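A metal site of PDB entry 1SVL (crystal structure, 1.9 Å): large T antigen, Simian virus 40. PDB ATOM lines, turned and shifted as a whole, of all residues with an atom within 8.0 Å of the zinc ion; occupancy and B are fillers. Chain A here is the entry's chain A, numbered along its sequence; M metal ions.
Of the 21 residues printed, 4 come within 4 Å of the zinc ion. The nearest printed residue that does not touch the zinc ion is Lys 54 (4.4 Å).
NE2 of His 67 is in hydrogen-bond range of O of Phe 45. A ring nitrogen (NE2) of His 67 is in hydrogen-bond range of the backbone carbonyl oxygen of Tyr 47, 2.7 Å away. A ring nitrogen (ND1) of His 63 is in hydrogen-bond range of the side-chain carboxylate (OE1) of Glu 44 (3.1 Å). SG of Cys 52 lies close to N of Lys 54, 3.5 Å away.
The zinc ion is bound by ND1 of His 67 (2.0 Å), NE2 of His 63 (2.2 Å), SG of Cys 55 (2.2 Å) and SG of Cys 52 (2.3 Å).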
ATOM      1  N   GLU A  44     -20.974  29.453 -22.266  1.00  0.00           N
ATOM      2  CA  GLU A  44     -20.430  29.985 -21.019  1.00  0.00           C
ATOM      3  C   GLU A  44     -18.921  29.821 -20.952  1.00  0.00           C
ATOM      4  O   GLU A  44     -18.280  30.378 -20.066  1.00  0.00           O
ATOM      5  CB  GLU A  44     -21.005  29.256 -19.787  1.00  0.00           C
ATOM      6  CG  GLU A  44     -22.513  29.224 -19.704  1.00  0.00           C
ATOM      7  CD  GLU A  44     -23.020  28.650 -18.384  1.00  0.00           C
ATOM      8  OE1 GLU A  44     -22.280  27.874 -17.736  1.00  0.00           O
ATOM      9  OE2 GLU A  44     -24.151  28.975 -17.987  1.00  0.00           O
ATOM     10  N   PHE A  45     -18.358  29.060 -21.877  1.00  0.00           N
ATOM     11  CA  PHE A  45     -16.918  28.866 -21.862  1.00  0.00           C
ATOM     12  C   PHE A  45     -16.203  29.895 -22.714  1.00  0.00           C
ATOM     13  O   PHE A  45     -14.963  29.930 -22.730  1.00  0.00           O
ATOM     14  CB  PHE A  45     -16.548  27.469 -22.385  1.00  0.00           C
ATOM     15  CG  PHE A  45     -17.153  26.342 -21.587  1.00  0.00           C
ATOM     16  CD1 PHE A  45     -17.328  26.451 -20.212  1.00  0.00           C
ATOM     17  CD2 PHE A  45     -17.488  25.148 -22.228  1.00  0.00           C
ATOM     18  CE1 PHE A  45     -17.839  25.386 -19.466  1.00  0.00           C
ATOM     19  CE2 PHE A  45     -17.995  24.068 -21.509  1.00  0.00           C
ATOM     20  CZ  PHE A  45     -18.162  24.182 -20.113  1.00  0.00           C
ATOM     21  N   GLN A  46     -16.960  30.719 -23.417  1.00  0.00           N
ATOM     22  CA  GLN A  46     -16.361  31.717 -24.297  1.00  0.00           C
ATOM     23  C   GLN A  46     -15.611  32.805 -23.535  1.00  0.00           C
ATOM     24  O   GLN A  46     -14.661  33.380 -24.068  1.00  0.00           O
ATOM     25  CB  GLN A  46     -17.445  32.372 -25.172  1.00  0.00           C
ATOM     26  CG  GLN A  46     -18.261  33.436 -24.455  1.00  0.00           C
ATOM     27  CD  GLN A  46     -19.398  33.951 -25.320  1.00  0.00           C
ATOM     28  OE1 GLN A  46     -20.516  33.424 -25.269  1.00  0.00           O
ATOM     29  NE2 GLN A  46     -19.121  34.949 -26.131  1.00  0.00           N
ATOM     30  N   TYR A  47     -16.040  33.083 -22.310  1.00  0.00           N
ATOM     31  CA  TYR A  47     -15.436  34.116 -21.478  1.00  0.00           C
ATOM     32  C   TYR A  47     -14.151  33.622 -20.809  1.00  0.00           C
ATOM     33  O   TYR A  47     -13.959  32.409 -20.667  1.00  0.00           O
ATOM     34  CB  TYR A  47     -16.454  34.570 -20.439  1.00  0.00           C
ATOM     35  CG  TYR A  47     -17.780  35.000 -21.066  1.00  0.00           C
ATOM     36  CD1 TYR A  47     -17.854  36.157 -21.840  1.00  0.00           C
ATOM     37  CD2 TYR A  47     -18.930  34.223 -20.907  1.00  0.00           C
ATOM     38  CE1 TYR A  47     -19.046  36.542 -22.452  1.00  0.00           C
ATOM     39  CE2 TYR A  47     -20.122  34.590 -21.507  1.00  0.00           C
ATOM     40  CZ  TYR A  47     -20.181  35.748 -22.271  1.00  0.00           C
ATOM     41  OH  TYR A  47     -21.363  36.099 -22.886  1.00  0.00           O
ATOM     42  N   SER A  48     -13.278  34.527 -20.391  1.00  0.00           N
ATOM     43  CA  SER A  48     -12.020  34.117 -19.775  1.00  0.00           C
ATOM     44  C   SER A  48     -12.242  33.178 -18.584  1.00  0.00           C
ATOM     45  O   SER A  48     -13.144  33.387 -17.768  1.00  0.00           O
ATOM     46  CB  SER A  48     -11.191  35.329 -19.340  1.00  0.00           C
ATOM     47  OG  SER A  48     -11.778  35.992 -18.229  1.00  0.00           O
ATOM     48  N   PHE A  49     -11.417  32.150 -18.496  1.00  0.00           N
ATOM     49  CA  PHE A  49     -11.481  31.194 -17.400  1.00  0.00           C
ATOM     50  C   PHE A  49     -10.806  31.751 -16.148  1.00  0.00           C
ATOM     51  O   PHE A  49     -11.141  31.361 -15.033  1.00  0.00           O
ATOM     52  CB  PHE A  49     -10.770  29.898 -17.794  1.00  0.00           C
ATOM     53  CG  PHE A  49     -10.431  29.037 -16.615  1.00  0.00           C
ATOM     54  CD1 PHE A  49     -11.446  28.529 -15.793  1.00  0.00           C
ATOM     55  CD2 PHE A  49      -9.109  28.776 -16.292  1.00  0.00           C
ATOM     56  CE1 PHE A  49     -11.148  27.776 -14.656  1.00  0.00           C
ATOM     57  CE2 PHE A  49      -8.778  28.029 -15.154  1.00  0.00           C
ATOM     58  CZ  PHE A  49      -9.806  27.526 -14.332  1.00  0.00           C
ATOM     59  N   GLU A  50      -9.848  32.656 -16.344  1.00  0.00           N
ATOM     60  CA  GLU A  50      -9.114  33.287 -15.244  1.00  0.00           C
ATOM     61  C   GLU A  50      -9.979  34.205 -14.377  1.00  0.00           C
ATOM     62  O   GLU A  50      -9.735  34.356 -13.183  1.00  0.00           O
ATOM     63  CB  GLU A  50      -7.945  34.099 -15.805  1.00  0.00           C
ATOM     64  CG  GLU A  50      -6.945  33.273 -16.579  1.00  0.00           C
ATOM     65  CD  GLU A  50      -6.126  32.361 -15.690  1.00  0.00           C
ATOM     66  OE1 GLU A  50      -6.717  31.543 -14.951  1.00  0.00           O
ATOM     67  OE2 GLU A  50      -4.880  32.468 -15.721  1.00  0.00           O
ATOM     68  N   MET A  51     -10.963  34.839 -14.986  1.00  0.00           N
ATOM     69  CA  MET A  51     -11.833  35.744 -14.246  1.00  0.00           C
ATOM     70  C   MET A  51     -13.278  35.254 -14.324  1.00  0.00           C
ATOM     71  O   MET A  51     -14.197  36.023 -14.632  1.00  0.00           O
ATOM     72  CB  MET A  51     -11.746  37.152 -14.833  1.00  0.00           C
ATOM     73  CG  MET A  51     -10.321  37.660 -14.947  1.00  0.00           C
ATOM     74  SD  MET A  51     -10.210  39.207 -15.849  1.00  0.00           S
ATOM     75  CE  MET A  51     -10.068  38.629 -17.533  1.00  0.00           C
ATOM     76  N   CYS A  52     -13.455  33.967 -14.039  1.00  0.00           N
ATOM     77  CA  CYS A  52     -14.782  33.352 -14.093  1.00  0.00           C
ATOM     78  C   CYS A  52     -15.424  33.126 -12.729  1.00  0.00           C
ATOM     79  O   CYS A  52     -14.980  32.311 -11.928  1.00  0.00           O
ATOM     80  CB  CYS A  52     -14.701  32.005 -14.825  1.00  0.00           C
ATOM     81  SG  CYS A  52     -16.332  31.304 -15.064  1.00  0.00           S
ATOM     82  N   LEU A  53     -16.509  33.857 -12.478  1.00  0.00           N
ATOM     83  CA  LEU A  53     -17.229  33.727 -11.227  1.00  0.00           C
ATOM     84  C   LEU A  53     -17.732  32.302 -11.061  1.00  0.00           C
ATOM     85  O   LEU A  53     -17.651  31.748  -9.969  1.00  0.00           O
ATOM     86  CB  LEU A  53     -18.428  34.682 -11.209  1.00  0.00           C
ATOM     87  CG  LEU A  53     -19.323  34.593  -9.963  1.00  0.00           C
ATOM     88  CD1 LEU A  53     -18.514  35.000  -8.746  1.00  0.00           C
ATOM     89  CD2 LEU A  53     -20.531  35.518 -10.120  1.00  0.00           C
ATOM     90  N   LYS A  54     -18.227  31.705 -12.136  1.00  0.00           N
ATOM     91  CA  LYS A  54     -18.762  30.341 -12.055  1.00  0.00           C
ATOM     92  C   LYS A  54     -17.704  29.329 -11.681  1.00  0.00           C
ATOM     93  O   LYS A  54     -17.983  28.398 -10.929  1.00  0.00           O
ATOM     94  CB  LYS A  54     -19.449  29.923 -13.365  1.00  0.00           C
ATOM     95  CG  LYS A  54     -20.673  30.765 -13.696  1.00  0.00           C
ATOM     96  CD  LYS A  54     -21.576  30.131 -14.745  1.00  0.00           C
ATOM     97  CE  LYS A  54     -22.485  29.036 -14.128  1.00  0.00           C
ATOM     98  NZ  LYS A  54     -21.795  27.789 -13.622  1.00  0.00           N
ATOM     99  N   CYS A  55     -16.489  29.488 -12.189  1.00  0.00           N
ATOM    100  CA  CYS A  55     -15.423  28.553 -11.845  1.00  0.00           C
ATOM    101  C   CYS A  55     -14.902  28.806 -10.435  1.00  0.00           C
ATOM    102  O   CYS A  55     -14.625  27.862  -9.693  1.00  0.00           O
ATOM    103  CB  CYS A  55     -14.261  28.644 -12.840  1.00  0.00           C
ATOM    104  SG  CYS A  55     -14.541  27.826 -14.414  1.00  0.00           S
ATOM    105  N   ILE A  56     -14.776  30.075 -10.038  1.00  0.00           N
ATOM    106  CA  ILE A  56     -14.263  30.355  -8.707  1.00  0.00           C
ATOM    107  C   ILE A  56     -15.238  29.911  -7.615  1.00  0.00           C
ATOM    108  O   ILE A  56     -14.827  29.509  -6.539  1.00  0.00           O
ATOM    109  CB  ILE A  56     -13.930  31.863  -8.523  1.00  0.00           C
ATOM    110  CG1 ILE A  56     -13.201  32.092  -7.201  1.00  0.00           C
ATOM    111  CG2 ILE A  56     -15.194  32.700  -8.532  1.00  0.00           C
ATOM    112  CD1 ILE A  56     -11.914  31.309  -7.074  1.00  0.00           C
ATOM    113  N   LYS A  57     -16.542  29.969  -7.886  1.00  0.00           N
ATOM    114  CA  LYS A  57     -17.528  29.564  -6.894  1.00  0.00           C
ATOM    115  C   LYS A  57     -17.823  28.057  -6.938  1.00  0.00           C
ATOM    116  O   LYS A  57     -18.519  27.540  -6.066  1.00  0.00           O
ATOM    117  CB  LYS A  57     -18.828  30.363  -7.067  1.00  0.00           C
ATOM    118  CG  LYS A  57     -18.735  31.841  -6.700  1.00  0.00           C
ATOM    119  CD  LYS A  57     -20.119  32.379  -6.311  1.00  0.00           C
ATOM    120  CE  LYS A  57     -21.129  32.174  -7.429  1.00  0.00           C
ATOM    121  NZ  LYS A  57     -22.477  32.669  -7.017  1.00  0.00           N
ATOM    122  N   GLN A  60     -21.197  24.637 -10.701  1.00  0.00           N
ATOM    123  CA  GLN A  60     -21.590  23.451 -11.470  1.00  0.00           C
ATOM    124  C   GLN A  60     -20.395  22.703 -12.080  1.00  0.00           C
ATOM    125  O   GLN A  60     -19.665  23.257 -12.899  1.00  0.00           O
ATOM    126  CB  GLN A  60     -22.553  23.852 -12.589  1.00  0.00           C
ATOM    127  CG  GLN A  60     -23.799  24.568 -12.095  1.00  0.00           C
ATOM    128  CD  GLN A  60     -24.773  23.603 -11.456  1.00  0.00           C
ATOM    129  OE1 GLN A  60     -25.671  24.013 -10.721  1.00  0.00           O
ATOM    130  NE2 GLN A  60     -24.607  22.324 -11.734  1.00  0.00           N
ATOM    131  N   HIS A  63     -19.654  22.688 -15.479  1.00  0.00           N
ATOM    132  CA  HIS A  63     -19.079  23.937 -15.972  1.00  0.00           C
ATOM    133  C   HIS A  63     -17.607  24.058 -15.602  1.00  0.00           C
ATOM    134  O   HIS A  63     -16.737  24.015 -16.477  1.00  0.00           O
ATOM    135  CB  HIS A  63     -19.796  25.183 -15.392  1.00  0.00           C
ATOM    136  CG  HIS A  63     -19.125  26.465 -15.768  1.00  0.00           C
ATOM    137  ND1 HIS A  63     -19.336  27.098 -16.975  1.00  0.00           N
ATOM    138  CD2 HIS A  63     -18.178  27.198 -15.120  1.00  0.00           C
ATOM    139  CE1 HIS A  63     -18.550  28.163 -17.060  1.00  0.00           C
ATOM    140  NE2 HIS A  63     -17.844  28.243 -15.951  1.00  0.00           N
ATOM    141  N   TYR A  64     -17.320  24.176 -14.307  1.00  0.00           N
ATOM    142  CA  TYR A  64     -15.946  24.373 -13.845  1.00  0.00           C
ATOM    143  C   TYR A  64     -14.914  23.297 -14.152  1.00  0.00           C
ATOM    144  O   TYR A  64     -13.722  23.579 -14.207  1.00  0.00           O
ATOM    145  CB  TYR A  64     -15.933  24.717 -12.339  1.00  0.00           C
ATOM    146  CG  TYR A  64     -16.326  23.611 -11.378  1.00  0.00           C
ATOM    147  CD1 TYR A  64     -15.441  22.570 -11.083  1.00  0.00           C
ATOM    148  CD2 TYR A  64     -17.536  23.675 -10.669  1.00  0.00           C
ATOM    149  CE1 TYR A  64     -15.739  21.638 -10.116  1.00  0.00           C
ATOM    150  CE2 TYR A  64     -17.840  22.745  -9.714  1.00  0.00           C
ATOM    151  CZ  TYR A  64     -16.940  21.723  -9.423  1.00  0.00           C
ATOM    152  OH  TYR A  64     -17.226  20.825  -8.432  1.00  0.00           O
ATOM    153  N   LYS A  65     -15.364  22.074 -14.399  1.00  0.00           N
ATOM    154  CA  LYS A  65     -14.440  21.007 -14.740  1.00  0.00           C
ATOM    155  C   LYS A  65     -14.027  21.114 -16.194  1.00  0.00           C
ATOM    156  O   LYS A  65     -13.038  20.528 -16.613  1.00  0.00           O
ATOM    157  CB  LYS A  65     -15.077  19.635 -14.507  1.00  0.00           C
ATOM    158  CG  LYS A  65     -15.094  19.173 -13.049  1.00  0.00           C
ATOM    159  CD  LYS A  65     -13.686  18.883 -12.550  1.00  0.00           C
ATOM    160  CE  LYS A  65     -13.691  18.180 -11.186  1.00  0.00           C
ATOM    161  NZ  LYS A  65     -14.535  16.950 -11.195  1.00  0.00           N
ATOM    162  N   TYR A  66     -14.778  21.879 -16.982  1.00  0.00           N
ATOM    163  CA  TYR A  66     -14.448  21.975 -18.398  1.00  0.00           C
ATOM    164  C   TYR A  66     -14.138  23.329 -19.007  1.00  0.00           C
ATOM    165  O   TYR A  66     -13.598  23.383 -20.103  1.00  0.00           O
ATOM    166  CB  TYR A  66     -15.581  21.347 -19.216  1.00  0.00           C
ATOM    167  CG  TYR A  66     -15.929  19.942 -18.811  1.00  0.00           C
ATOM    168  CD1 TYR A  66     -16.846  19.703 -17.802  1.00  0.00           C
ATOM    169  CD2 TYR A  66     -15.339  18.855 -19.438  1.00  0.00           C
ATOM    170  CE1 TYR A  66     -17.174  18.408 -17.429  1.00  0.00           C
ATOM    171  CE2 TYR A  66     -15.653  17.554 -19.089  1.00  0.00           C
ATOM    172  CZ  TYR A  66     -16.575  17.341 -18.072  1.00  0.00           C
ATOM    173  OH  TYR A  66     -16.894  16.048 -17.703  1.00  0.00           O
ATOM    174  N   HIS A  67     -14.488  24.419 -18.322  1.00  0.00           N
ATOM    175  CA  HIS A  67     -14.266  25.770 -18.873  1.00  0.00           C
ATOM    176  C   HIS A  67     -12.845  25.987 -19.415  1.00  0.00           C
ATOM    177  O   HIS A  67     -12.676  26.309 -20.597  1.00  0.00           O
ATOM    178  CB  HIS A  67     -14.587  26.813 -17.788  1.00  0.00           C
ATOM    179  CG  HIS A  67     -14.678  28.222 -18.288  1.00  0.00           C
ATOM    180  ND1 HIS A  67     -15.037  29.269 -17.471  1.00  0.00           N
ATOM    181  CD2 HIS A  67     -14.462  28.761 -19.520  1.00  0.00           C
ATOM    182  CE1 HIS A  67     -15.026  30.400 -18.170  1.00  0.00           C
ATOM    183  NE2 HIS A  67     -14.681  30.118 -19.410  1.00  0.00           N
ATOM    184  N   GLU A  68     -11.831  25.784 -18.583  1.00  0.00           N
ATOM    185  CA  GLU A  68     -10.461  26.022 -19.018  1.00  0.00           C
ATOM    186  C   GLU A  68     -10.096  25.250 -20.278  1.00  0.00           C
ATOM    187  O   GLU A  68      -9.549  25.803 -21.231  1.00  0.00           O
ATOM    188  CB  GLU A  68      -9.476  25.700 -17.897  1.00  0.00           C
ATOM    189  CG  GLU A  68      -8.023  26.013 -18.241  1.00  0.00           C
ATOM    190  CD  GLU A  68      -7.080  25.787 -17.067  1.00  0.00           C
ATOM    191  OE1 GLU A  68      -6.976  24.626 -16.595  1.00  0.00           O
ATOM    192  OE2 GLU A  68      -6.457  26.758 -16.604  1.00  0.00           O
HETATM  193 ZN    ZN M   1     -15.842  29.130 -15.687  1.00  0.00          ZN
